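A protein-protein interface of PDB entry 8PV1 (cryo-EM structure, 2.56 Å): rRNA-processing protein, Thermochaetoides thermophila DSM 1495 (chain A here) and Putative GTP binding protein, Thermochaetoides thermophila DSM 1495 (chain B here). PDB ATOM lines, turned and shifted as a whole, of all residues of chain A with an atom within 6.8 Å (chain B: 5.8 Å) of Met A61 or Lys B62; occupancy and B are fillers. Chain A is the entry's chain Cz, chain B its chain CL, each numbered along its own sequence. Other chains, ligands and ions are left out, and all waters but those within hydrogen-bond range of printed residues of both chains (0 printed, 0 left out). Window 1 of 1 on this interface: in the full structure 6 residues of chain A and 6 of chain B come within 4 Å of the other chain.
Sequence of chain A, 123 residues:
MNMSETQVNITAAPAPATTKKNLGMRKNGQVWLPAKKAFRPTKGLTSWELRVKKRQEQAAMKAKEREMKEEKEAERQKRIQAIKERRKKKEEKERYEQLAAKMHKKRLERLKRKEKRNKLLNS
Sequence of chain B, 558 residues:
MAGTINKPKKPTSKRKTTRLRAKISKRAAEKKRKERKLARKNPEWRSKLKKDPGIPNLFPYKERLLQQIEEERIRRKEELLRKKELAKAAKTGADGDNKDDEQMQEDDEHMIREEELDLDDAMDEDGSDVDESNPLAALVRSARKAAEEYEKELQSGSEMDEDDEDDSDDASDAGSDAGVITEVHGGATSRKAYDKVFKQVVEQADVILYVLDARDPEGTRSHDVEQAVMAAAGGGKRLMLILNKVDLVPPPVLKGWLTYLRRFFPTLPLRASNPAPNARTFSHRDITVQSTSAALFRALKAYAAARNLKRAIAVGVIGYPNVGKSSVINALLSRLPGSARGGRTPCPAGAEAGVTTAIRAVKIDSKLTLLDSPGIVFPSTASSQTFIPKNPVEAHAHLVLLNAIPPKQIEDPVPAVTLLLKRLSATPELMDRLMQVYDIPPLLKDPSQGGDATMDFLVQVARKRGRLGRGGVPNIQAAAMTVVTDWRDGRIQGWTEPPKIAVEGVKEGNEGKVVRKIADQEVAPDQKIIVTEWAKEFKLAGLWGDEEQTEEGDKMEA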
ATOM      1  N   GLN A  56      23.422 -16.110  11.244  1.00  0.00           N
ATOM      2  CA  GLN A  56      22.342 -17.022  10.866  1.00  0.00           C
ATOM      3  C   GLN A  56      21.956 -17.936  12.024  1.00  0.00           C
ATOM      4  O   GLN A  56      20.765 -18.114  12.325  1.00  0.00           O
ATOM      5  CB  GLN A  56      22.756 -17.847   9.651  1.00  0.00           C
ATOM      6  CG  GLN A  56      23.022 -17.018   8.420  1.00  0.00           C
ATOM      7  CD  GLN A  56      23.551 -17.841   7.265  1.00  0.00           C
ATOM      8  OE1 GLN A  56      24.301 -18.800   7.461  1.00  0.00           O
ATOM      9  NE2 GLN A  56      23.168 -17.467   6.051  1.00  0.00           N
ATOM     10  N   GLU A  57      22.959 -18.506  12.701  1.00  0.00           N
ATOM     11  CA  GLU A  57      22.684 -19.377  13.842  1.00  0.00           C
ATOM     12  C   GLU A  57      22.008 -18.612  14.976  1.00  0.00           C
ATOM     13  O   GLU A  57      21.087 -19.129  15.625  1.00  0.00           O
ATOM     14  CB  GLU A  57      23.980 -20.024  14.330  1.00  0.00           C
ATOM     15  CG  GLU A  57      24.629 -20.950  13.315  1.00  0.00           C
ATOM     16  CD  GLU A  57      25.996 -21.436  13.751  1.00  0.00           C
ATOM     17  OE1 GLU A  57      26.502 -20.961  14.790  1.00  0.00           O
ATOM     18  OE2 GLU A  57      26.561 -22.306  13.058  1.00  0.00           O
ATOM     19  N   GLN A  58      22.447 -17.371  15.214  1.00  0.00           N
ATOM     20  CA  GLN A  58      21.887 -16.529  16.265  1.00  0.00           C
ATOM     21  C   GLN A  58      20.428 -16.196  15.986  1.00  0.00           C
ATOM     22  O   GLN A  58      19.585 -16.279  16.889  1.00  0.00           O
ATOM     23  CB  GLN A  58      22.719 -15.249  16.368  1.00  0.00           C
ATOM     24  CG  GLN A  58      22.338 -14.274  17.468  1.00  0.00           C
ATOM     25  CD  GLN A  58      22.593 -14.825  18.853  1.00  0.00           C
ATOM     26  OE1 GLN A  58      23.613 -15.469  19.099  1.00  0.00           O
ATOM     27  NE2 GLN A  58      21.687 -14.540  19.776  1.00  0.00           N
ATOM     28  N   ALA A  59      20.111 -15.842  14.735  1.00  0.00           N
ATOM     29  CA  ALA A  59      18.732 -15.530  14.374  1.00  0.00           C
ATOM     30  C   ALA A  59      17.835 -16.753  14.502  1.00  0.00           C
ATOM     31  O   ALA A  59      16.710 -16.651  15.007  1.00  0.00           O
ATOM     32  CB  ALA A  59      18.668 -14.966  12.954  1.00  0.00           C
ATOM     33  N   ALA A  60      18.323 -17.923  14.069  1.00  0.00           N
ATOM     34  CA  ALA A  60      17.527 -19.145  14.175  1.00  0.00           C
ATOM     35  C   ALA A  60      17.247 -19.510  15.631  1.00  0.00           C
ATOM     36  O   ALA A  60      16.111 -19.855  15.992  1.00  0.00           O
ATOM     37  CB  ALA A  60      18.238 -20.290  13.455  1.00  0.00           C
ATOM     38  N   MET A  61      18.274 -19.428  16.487  1.00  0.00           N
ATOM     39  CA  MET A  61      18.086 -19.774  17.894  1.00  0.00           C
ATOM     40  C   MET A  61      17.154 -18.780  18.576  1.00  0.00           C
ATOM     41  O   MET A  61      16.311 -19.174  19.393  1.00  0.00           O
ATOM     42  CB  MET A  61      19.457 -19.879  18.584  1.00  0.00           C
ATOM     43  CG  MET A  61      19.549 -19.883  20.136  1.00  0.00           C
ATOM     44  SD  MET A  61      19.103 -18.444  21.151  1.00  0.00           S
ATOM     45  CE  MET A  61      20.586 -17.457  21.033  1.00  0.00           C
ATOM     46  N   LYS A  62      17.278 -17.487  18.247  1.00  0.00           N
ATOM     47  CA  LYS A  62      16.380 -16.490  18.828  1.00  0.00           C
ATOM     48  C   LYS A  62      14.936 -16.716  18.404  1.00  0.00           C
ATOM     49  O   LYS A  62      14.018 -16.581  19.223  1.00  0.00           O
ATOM     50  CB  LYS A  62      16.819 -15.076  18.450  1.00  0.00           C
ATOM     51  CG  LYS A  62      18.045 -14.580  19.182  1.00  0.00           C
ATOM     52  CD  LYS A  62      17.834 -14.648  20.684  1.00  0.00           C
ATOM     53  CE  LYS A  62      16.801 -13.643  21.157  1.00  0.00           C
ATOM     54  NZ  LYS A  62      16.611 -13.728  22.629  1.00  0.00           N
ATOM     55  N   ALA A  63      14.718 -17.060  17.131  1.00  0.00           N
ATOM     56  CA  ALA A  63      13.365 -17.336  16.659  1.00  0.00           C
ATOM     57  C   ALA A  63      12.767 -18.541  17.377  1.00  0.00           C
ATOM     58  O   ALA A  63      11.599 -18.518  17.786  1.00  0.00           O
ATOM     59  CB  ALA A  63      13.376 -17.555  15.147  1.00  0.00           C
ATOM     60  N   LYS A  64      13.570 -19.595  17.562  1.00  0.00           N
ATOM     61  CA  LYS A  64      13.091 -20.782  18.271  1.00  0.00           C
ATOM     62  C   LYS A  64      12.751 -20.477  19.728  1.00  0.00           C
ATOM     63  O   LYS A  64      11.724 -20.940  20.248  1.00  0.00           O
ATOM     64  CB  LYS A  64      14.138 -21.892  18.194  1.00  0.00           C
ATOM     65  CG  LYS A  64      13.812 -23.097  19.047  1.00  0.00           C
ATOM     66  CD  LYS A  64      14.945 -24.093  19.065  1.00  0.00           C
ATOM     67  CE  LYS A  64      14.573 -25.281  19.920  1.00  0.00           C
ATOM     68  NZ  LYS A  64      15.645 -26.299  19.957  1.00  0.00           N
ATOM     69  N   GLU A  65      13.603 -19.701  20.405  1.00  0.00           N
ATOM     70  CA  GLU A  65      13.343 -19.350  21.798  1.00  0.00           C
ATOM     71  C   GLU A  65      12.100 -18.476  21.931  1.00  0.00           C
ATOM     72  O   GLU A  65      11.311 -18.639  22.875  1.00  0.00           O
ATOM     73  CB  GLU A  65      14.566 -18.656  22.394  1.00  0.00           C
ATOM     74  CG  GLU A  65      14.455 -18.357  23.878  1.00  0.00           C
ATOM     75  CD  GLU A  65      15.514 -17.383  24.344  1.00  0.00           C
ATOM     76  OE1 GLU A  65      16.203 -16.805  23.479  1.00  0.00           O
ATOM     77  OE2 GLU A  65      15.648 -17.183  25.570  1.00  0.00           O
ATOM     78  N   ARG A  66      11.903 -17.555  20.981  1.00  0.00           N
ATOM     79  CA  ARG A  66      10.688 -16.747  20.953  1.00  0.00           C
ATOM     80  C   ARG A  66       9.450 -17.621  20.787  1.00  0.00           C
ATOM     81  O   ARG A  66       8.438 -17.411  21.472  1.00  0.00           O
ATOM     82  CB  ARG A  66      10.783 -15.715  19.827  1.00  0.00           C
ATOM     83  CG  ARG A  66       9.625 -14.732  19.757  1.00  0.00           C
ATOM     84  CD  ARG A  66       9.826 -13.723  18.627  1.00  0.00           C
ATOM     85  NE  ARG A  66      10.989 -12.867  18.840  1.00  0.00           N
ATOM     86  CZ  ARG A  66      12.087 -12.888  18.099  1.00  0.00           C
ATOM     87  NH1 ARG A  66      12.223 -13.725  17.084  1.00  0.00           N
ATOM     88  NH2 ARG A  66      13.080 -12.049  18.387  1.00  0.00           N
ATOM     89  N   LYS A  69       8.784 -19.576  24.154  1.00  0.00           N
ATOM     90  CA  LYS A  69       8.164 -18.638  25.084  1.00  0.00           C
ATOM     91  C   LYS A  69       6.707 -18.379  24.726  1.00  0.00           C
ATOM     92  O   LYS A  69       5.866 -18.213  25.618  1.00  0.00           O
ATOM     93  CB  LYS A  69       8.945 -17.328  25.107  1.00  0.00           C
ATOM     94  CG  LYS A  69      10.267 -17.428  25.816  1.00  0.00           C
ATOM     95  CD  LYS A  69      11.003 -16.118  25.733  1.00  0.00           C
ATOM     96  CE  LYS A  69      12.197 -16.133  26.654  1.00  0.00           C
ATOM     97  NZ  LYS A  69      12.975 -14.880  26.548  1.00  0.00           N
ATOM     98  N   ILE B  55      18.681 -18.268  29.816  1.00  0.00           N
ATOM     99  CA  ILE B  55      19.975 -18.664  29.264  1.00  0.00           C
ATOM    100  C   ILE B  55      20.555 -17.475  28.507  1.00  0.00           C
ATOM    101  O   ILE B  55      19.828 -16.845  27.725  1.00  0.00           O
ATOM    102  CB  ILE B  55      19.835 -19.885  28.337  1.00  0.00           C
ATOM    103  CG1 ILE B  55      18.966 -20.952  28.998  1.00  0.00           C
ATOM    104  CG2 ILE B  55      21.199 -20.453  27.976  1.00  0.00           C
ATOM    105  CD1 ILE B  55      18.375 -21.939  28.027  1.00  0.00           C
ATOM    106  N   PRO B  56      21.825 -17.124  28.719  1.00  0.00           N
ATOM    107  CA  PRO B  56      22.419 -15.999  27.981  1.00  0.00           C
ATOM    108  C   PRO B  56      22.520 -16.295  26.492  1.00  0.00           C
ATOM    109  O   PRO B  56      22.708 -17.441  26.080  1.00  0.00           O
ATOM    110  CB  PRO B  56      23.803 -15.846  28.623  1.00  0.00           C
ATOM    111  CG  PRO B  56      23.689 -16.512  29.951  1.00  0.00           C
ATOM    112  CD  PRO B  56      22.735 -17.642  29.750  1.00  0.00           C
ATOM    113  N   ASN B  57      22.392 -15.241  25.683  1.00  0.00           N
ATOM    114  CA  ASN B  57      22.410 -15.411  24.233  1.00  0.00           C
ATOM    115  C   ASN B  57      23.810 -15.730  23.724  1.00  0.00           C
ATOM    116  O   ASN B  57      23.968 -16.422  22.712  1.00  0.00           O
ATOM    117  CB  ASN B  57      21.867 -14.156  23.551  1.00  0.00           C
ATOM    118  CG  ASN B  57      20.390 -13.951  23.805  1.00  0.00           C
ATOM    119  OD1 ASN B  57      19.655 -14.903  24.060  1.00  0.00           O
ATOM    120  ND2 ASN B  57      19.945 -12.702  23.732  1.00  0.00           N
ATOM    121  N   PHE B  59      25.996 -17.606  25.075  1.00  0.00           N
ATOM    122  CA  PHE B  59      26.359 -18.990  25.332  1.00  0.00           C
ATOM    123  C   PHE B  59      26.254 -19.797  24.038  1.00  0.00           C
ATOM    124  O   PHE B  59      25.182 -19.815  23.413  1.00  0.00           O
ATOM    125  CB  PHE B  59      25.455 -19.580  26.412  1.00  0.00           C
ATOM    126  CG  PHE B  59      25.830 -20.972  26.824  1.00  0.00           C
ATOM    127  CD1 PHE B  59      27.052 -21.225  27.422  1.00  0.00           C
ATOM    128  CD2 PHE B  59      24.956 -22.028  26.628  1.00  0.00           C
ATOM    129  CE1 PHE B  59      27.404 -22.505  27.802  1.00  0.00           C
ATOM    130  CE2 PHE B  59      25.299 -23.311  27.008  1.00  0.00           C
ATOM    131  CZ  PHE B  59      26.525 -23.548  27.595  1.00  0.00           C
ATOM    132  N   PRO B  60      27.332 -20.454  23.599  1.00  0.00           N
ATOM    133  CA  PRO B  60      27.325 -21.099  22.274  1.00  0.00           C
ATOM    134  C   PRO B  60      26.368 -22.274  22.139  1.00  0.00           C
ATOM    135  O   PRO B  60      25.912 -22.548  21.024  1.00  0.00           O
ATOM    136  CB  PRO B  60      28.784 -21.551  22.098  1.00  0.00           C
ATOM    137  CG  PRO B  60      29.568 -20.741  23.081  1.00  0.00           C
ATOM    138  CD  PRO B  60      28.654 -20.528  24.241  1.00  0.00           C
ATOM    139  N   TYR B  61      26.045 -22.974  23.225  1.00  0.00           N
ATOM    140  CA  TYR B  61      25.267 -24.205  23.165  1.00  0.00           C
ATOM    141  C   TYR B  61      23.839 -24.011  23.671  1.00  0.00           C
ATOM    142  O   TYR B  61      23.184 -24.966  24.105  1.00  0.00           O
ATOM    143  CB  TYR B  61      25.990 -25.304  23.941  1.00  0.00           C
ATOM    144  CG  TYR B  61      27.426 -25.481  23.499  1.00  0.00           C
ATOM    145  CD1 TYR B  61      27.759 -25.488  22.149  1.00  0.00           C
ATOM    146  CD2 TYR B  61      28.453 -25.594  24.424  1.00  0.00           C
ATOM    147  CE1 TYR B  61      29.065 -25.633  21.732  1.00  0.00           C
ATOM    148  CE2 TYR B  61      29.772 -25.734  24.014  1.00  0.00           C
ATOM    149  CZ  TYR B  61      30.069 -25.752  22.663  1.00  0.00           C
ATOM    150  OH  TYR B  61      31.366 -25.891  22.224  1.00  0.00           O
ATOM    151  N   LYS B  62      23.339 -22.773  23.588  1.00  0.00           N
ATOM    152  CA  LYS B  62      21.974 -22.480  24.008  1.00  0.00           C
ATOM    153  C   LYS B  62      20.957 -23.210  23.138  1.00  0.00           C
ATOM    154  O   LYS B  62      19.949 -23.714  23.643  1.00  0.00           O
ATOM    155  CB  LYS B  62      21.733 -20.969  23.969  1.00  0.00           C
ATOM    156  CG  LYS B  62      20.318 -20.537  24.330  1.00  0.00           C
ATOM    157  CD  LYS B  62      20.234 -19.031  24.516  1.00  0.00           C
ATOM    158  CE  LYS B  62      18.835 -18.589  24.896  1.00  0.00           C
ATOM    159  NZ  LYS B  62      18.776 -17.130  25.175  1.00  0.00           N
ATOM    160  N   GLU B  63      21.213 -23.289  21.831  1.00  0.00           N
ATOM    161  CA  GLU B  63      20.249 -23.909  20.925  1.00  0.00           C
ATOM    162  C   GLU B  63      20.163 -25.414  21.149  1.00  0.00           C
ATOM    163  O   GLU B  63      19.067 -25.988  21.151  1.00  0.00           O
ATOM    164  CB  GLU B  63      20.617 -23.601  19.475  1.00  0.00           C
ATOM    165  CG  GLU B  63      19.624 -24.133  18.456  1.00  0.00           C
ATOM    166  CD  GLU B  63      20.001 -23.761  17.037  1.00  0.00           C
ATOM    167  OE1 GLU B  63      21.052 -23.109  16.860  1.00  0.00           O
ATOM    168  OE2 GLU B  63      19.245 -24.107  16.103  1.00  0.00           O
ATOM    169  N   ARG B  64      21.306 -26.075  21.352  1.00  0.00           N
ATOM    170  CA  ARG B  64      21.264 -27.506  21.634  1.00  0.00           C
ATOM    171  C   ARG B  64      20.690 -27.769  23.021  1.00  0.00           C
ATOM    172  O   ARG B  64      20.056 -28.806  23.249  1.00  0.00           O
ATOM    173  CB  ARG B  64      22.648 -28.144  21.475  1.00  0.00           C
ATOM    174  CG  ARG B  64      23.731 -27.678  22.415  1.00  0.00           C
ATOM    175  CD  ARG B  64      25.045 -28.386  22.115  1.00  0.00           C
ATOM    176  NE  ARG B  64      24.960 -29.807  22.421  1.00  0.00           N
ATOM    177  CZ  ARG B  64      25.826 -30.726  22.016  1.00  0.00           C
ATOM    178  NH1 ARG B  64      26.892 -30.407  21.298  1.00  0.00           N
ATOM    179  NH2 ARG B  64      25.612 -31.999  22.330  1.00  0.00           N
ATOM    180  N   LEU B  65      20.882 -26.831  23.953  1.00  0.00           N
ATOM    181  CA  LEU B  65      20.231 -26.939  25.257  1.00  0.00           C
ATOM    182  C   LEU B  65      18.712 -26.826  25.139  1.00  0.00           C
ATOM    183  O   LEU B  65      17.976 -27.527  25.841  1.00  0.00           O
ATOM    184  CB  LEU B  65      20.788 -25.873  26.197  1.00  0.00           C
ATOM    185  CG  LEU B  65      20.220 -25.791  27.613  1.00  0.00           C
ATOM    186  CD1 LEU B  65      20.421 -27.102  28.348  1.00  0.00           C
ATOM    187  CD2 LEU B  65      20.887 -24.656  28.372  1.00  0.00           C
ATOM    188  N   LEU B  66      18.226 -25.945  24.258  1.00  0.00           N
ATOM    189  CA  LEU B  66      16.787 -25.856  24.008  1.00  0.00           C
ATOM    190  C   LEU B  66      16.265 -27.117  23.323  1.00  0.00           C
ATOM    191  O   LEU B  66      15.142 -27.561  23.597  1.00  0.00           O
ATOM    192  CB  LEU B  66      16.467 -24.623  23.163  1.00  0.00           C
ATOM    193  CG  LEU B  66      16.717 -23.247  23.784  1.00  0.00           C
ATOM    194  CD1 LEU B  66      16.490 -22.143  22.765  1.00  0.00           C
ATOM    195  CD2 LEU B  66      15.853 -23.036  25.007  1.00  0.00           C
ATOM    196  N   GLN B  67      17.064 -27.687  22.413  1.00  0.00           N
ATOM    197  CA  GLN B  67      16.736 -28.979  21.809  1.00  0.00           C
ATOM    198  C   GLN B  67      16.568 -30.049  22.879  1.00  0.00           C
ATOM    199  O   GLN B  67      15.598 -30.822  22.862  1.00  0.00           O
ATOM    200  CB  GLN B  67      17.832 -29.396  20.825  1.00  0.00           C
ATOM    201  CG  GLN B  67      17.716 -28.818  19.425  1.00  0.00           C
ATOM    202  CD  GLN B  67      18.999 -28.964  18.625  1.00  0.00           C
ATOM    203  OE1 GLN B  67      19.913 -29.686  19.024  1.00  0.00           O
ATOM    204  NE2 GLN B  67      19.076 -28.269  17.496  1.00  0.00           N
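The side-chain amino group (NZ) of Lys B62 lies within salt-bridge range of the side-chain carboxylate (OE1) of Glu A65, 3.1 Å away.
The side-chain amino group (NZ) of Lys A64 sits close to the backbone NH (N) of Gln B67 (3.2 Å).
The side-chain amide oxygen of Asn B57 sits at hydrogen-bond distance from the side-chain amino group of Lys B62 (2.6 Å).
The backbone carbonyl oxygen (O) of Ile B55 sits at hydrogen-bond distance from the side-chain amino group (NZ) of Lys B62, 2.8 Å away.
OE2 of Glu A65 lies within salt-bridge range of NZ of Lys A69, at 3.7 Å.
NZ of Lys A62 is in salt-bridge range of OE1 of Glu A65 (3.2 Å).
Of the 12 printed residues of chain B, 5 touch a printed residue of chain A.
Hydrophobic or aromatic side chains of chain B within 4 Å of the printed part of chain A: Leu B66.
Of the 12 printed residues of chain A, 5 touch a printed residue of chain B.
Among the printed residues, 11 pairs touch across the chains.
Among the printed residues, Asp or Glu carboxylates within 4 Å of a Lys or Arg side-chain nitrogen of the other chain: Glu A65 with Lys B62.
Gln A58 touches Asn B57.
O of Asn B57 touches CE of Met A61, 3.9 Å away.
Lys B62 touches Met A61 (CD to SD, 3.6 Å).
CG of Met A61 touches CB of Glu B63 (3.9 Å).
NZ of Lys A62 touches OD1 of Asn B57 (3.6 Å).
Lys A64 touches Glu B63 (NZ to O, 3.6 Å).
Leu B66 touches Lys A64.
OE1 of Glu A65 touches OD1 of Asn B57 (3.98 Å).
Glu A65 touches Leu B66 (CB to CD1, 3.9998 Å).
Of the printed residues of chain B, Gln A58 touches Asn B57 (3.8 Å).
Of chain B, only Asn B57 (3.9 Å), Lys B62 (3.6 Å) and Glu B63 (3.9 Å) come within 4 Å of Met A61.
Ala A63 touches none of the printed residues of chain B.
Of the printed residues of chain A, Asn B57 touches Gln A58 (3.8 Å), Met A61 (3.9 Å), Lys A62 (3.6 Å) and Glu A65 (3.98 Å).
Of chain A, only Met A61 and Glu A65 come within 4 Å of Lys B62.
The nearest residue of chain B that does not touch Met A61 is Leu B66 (4.5 Å).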
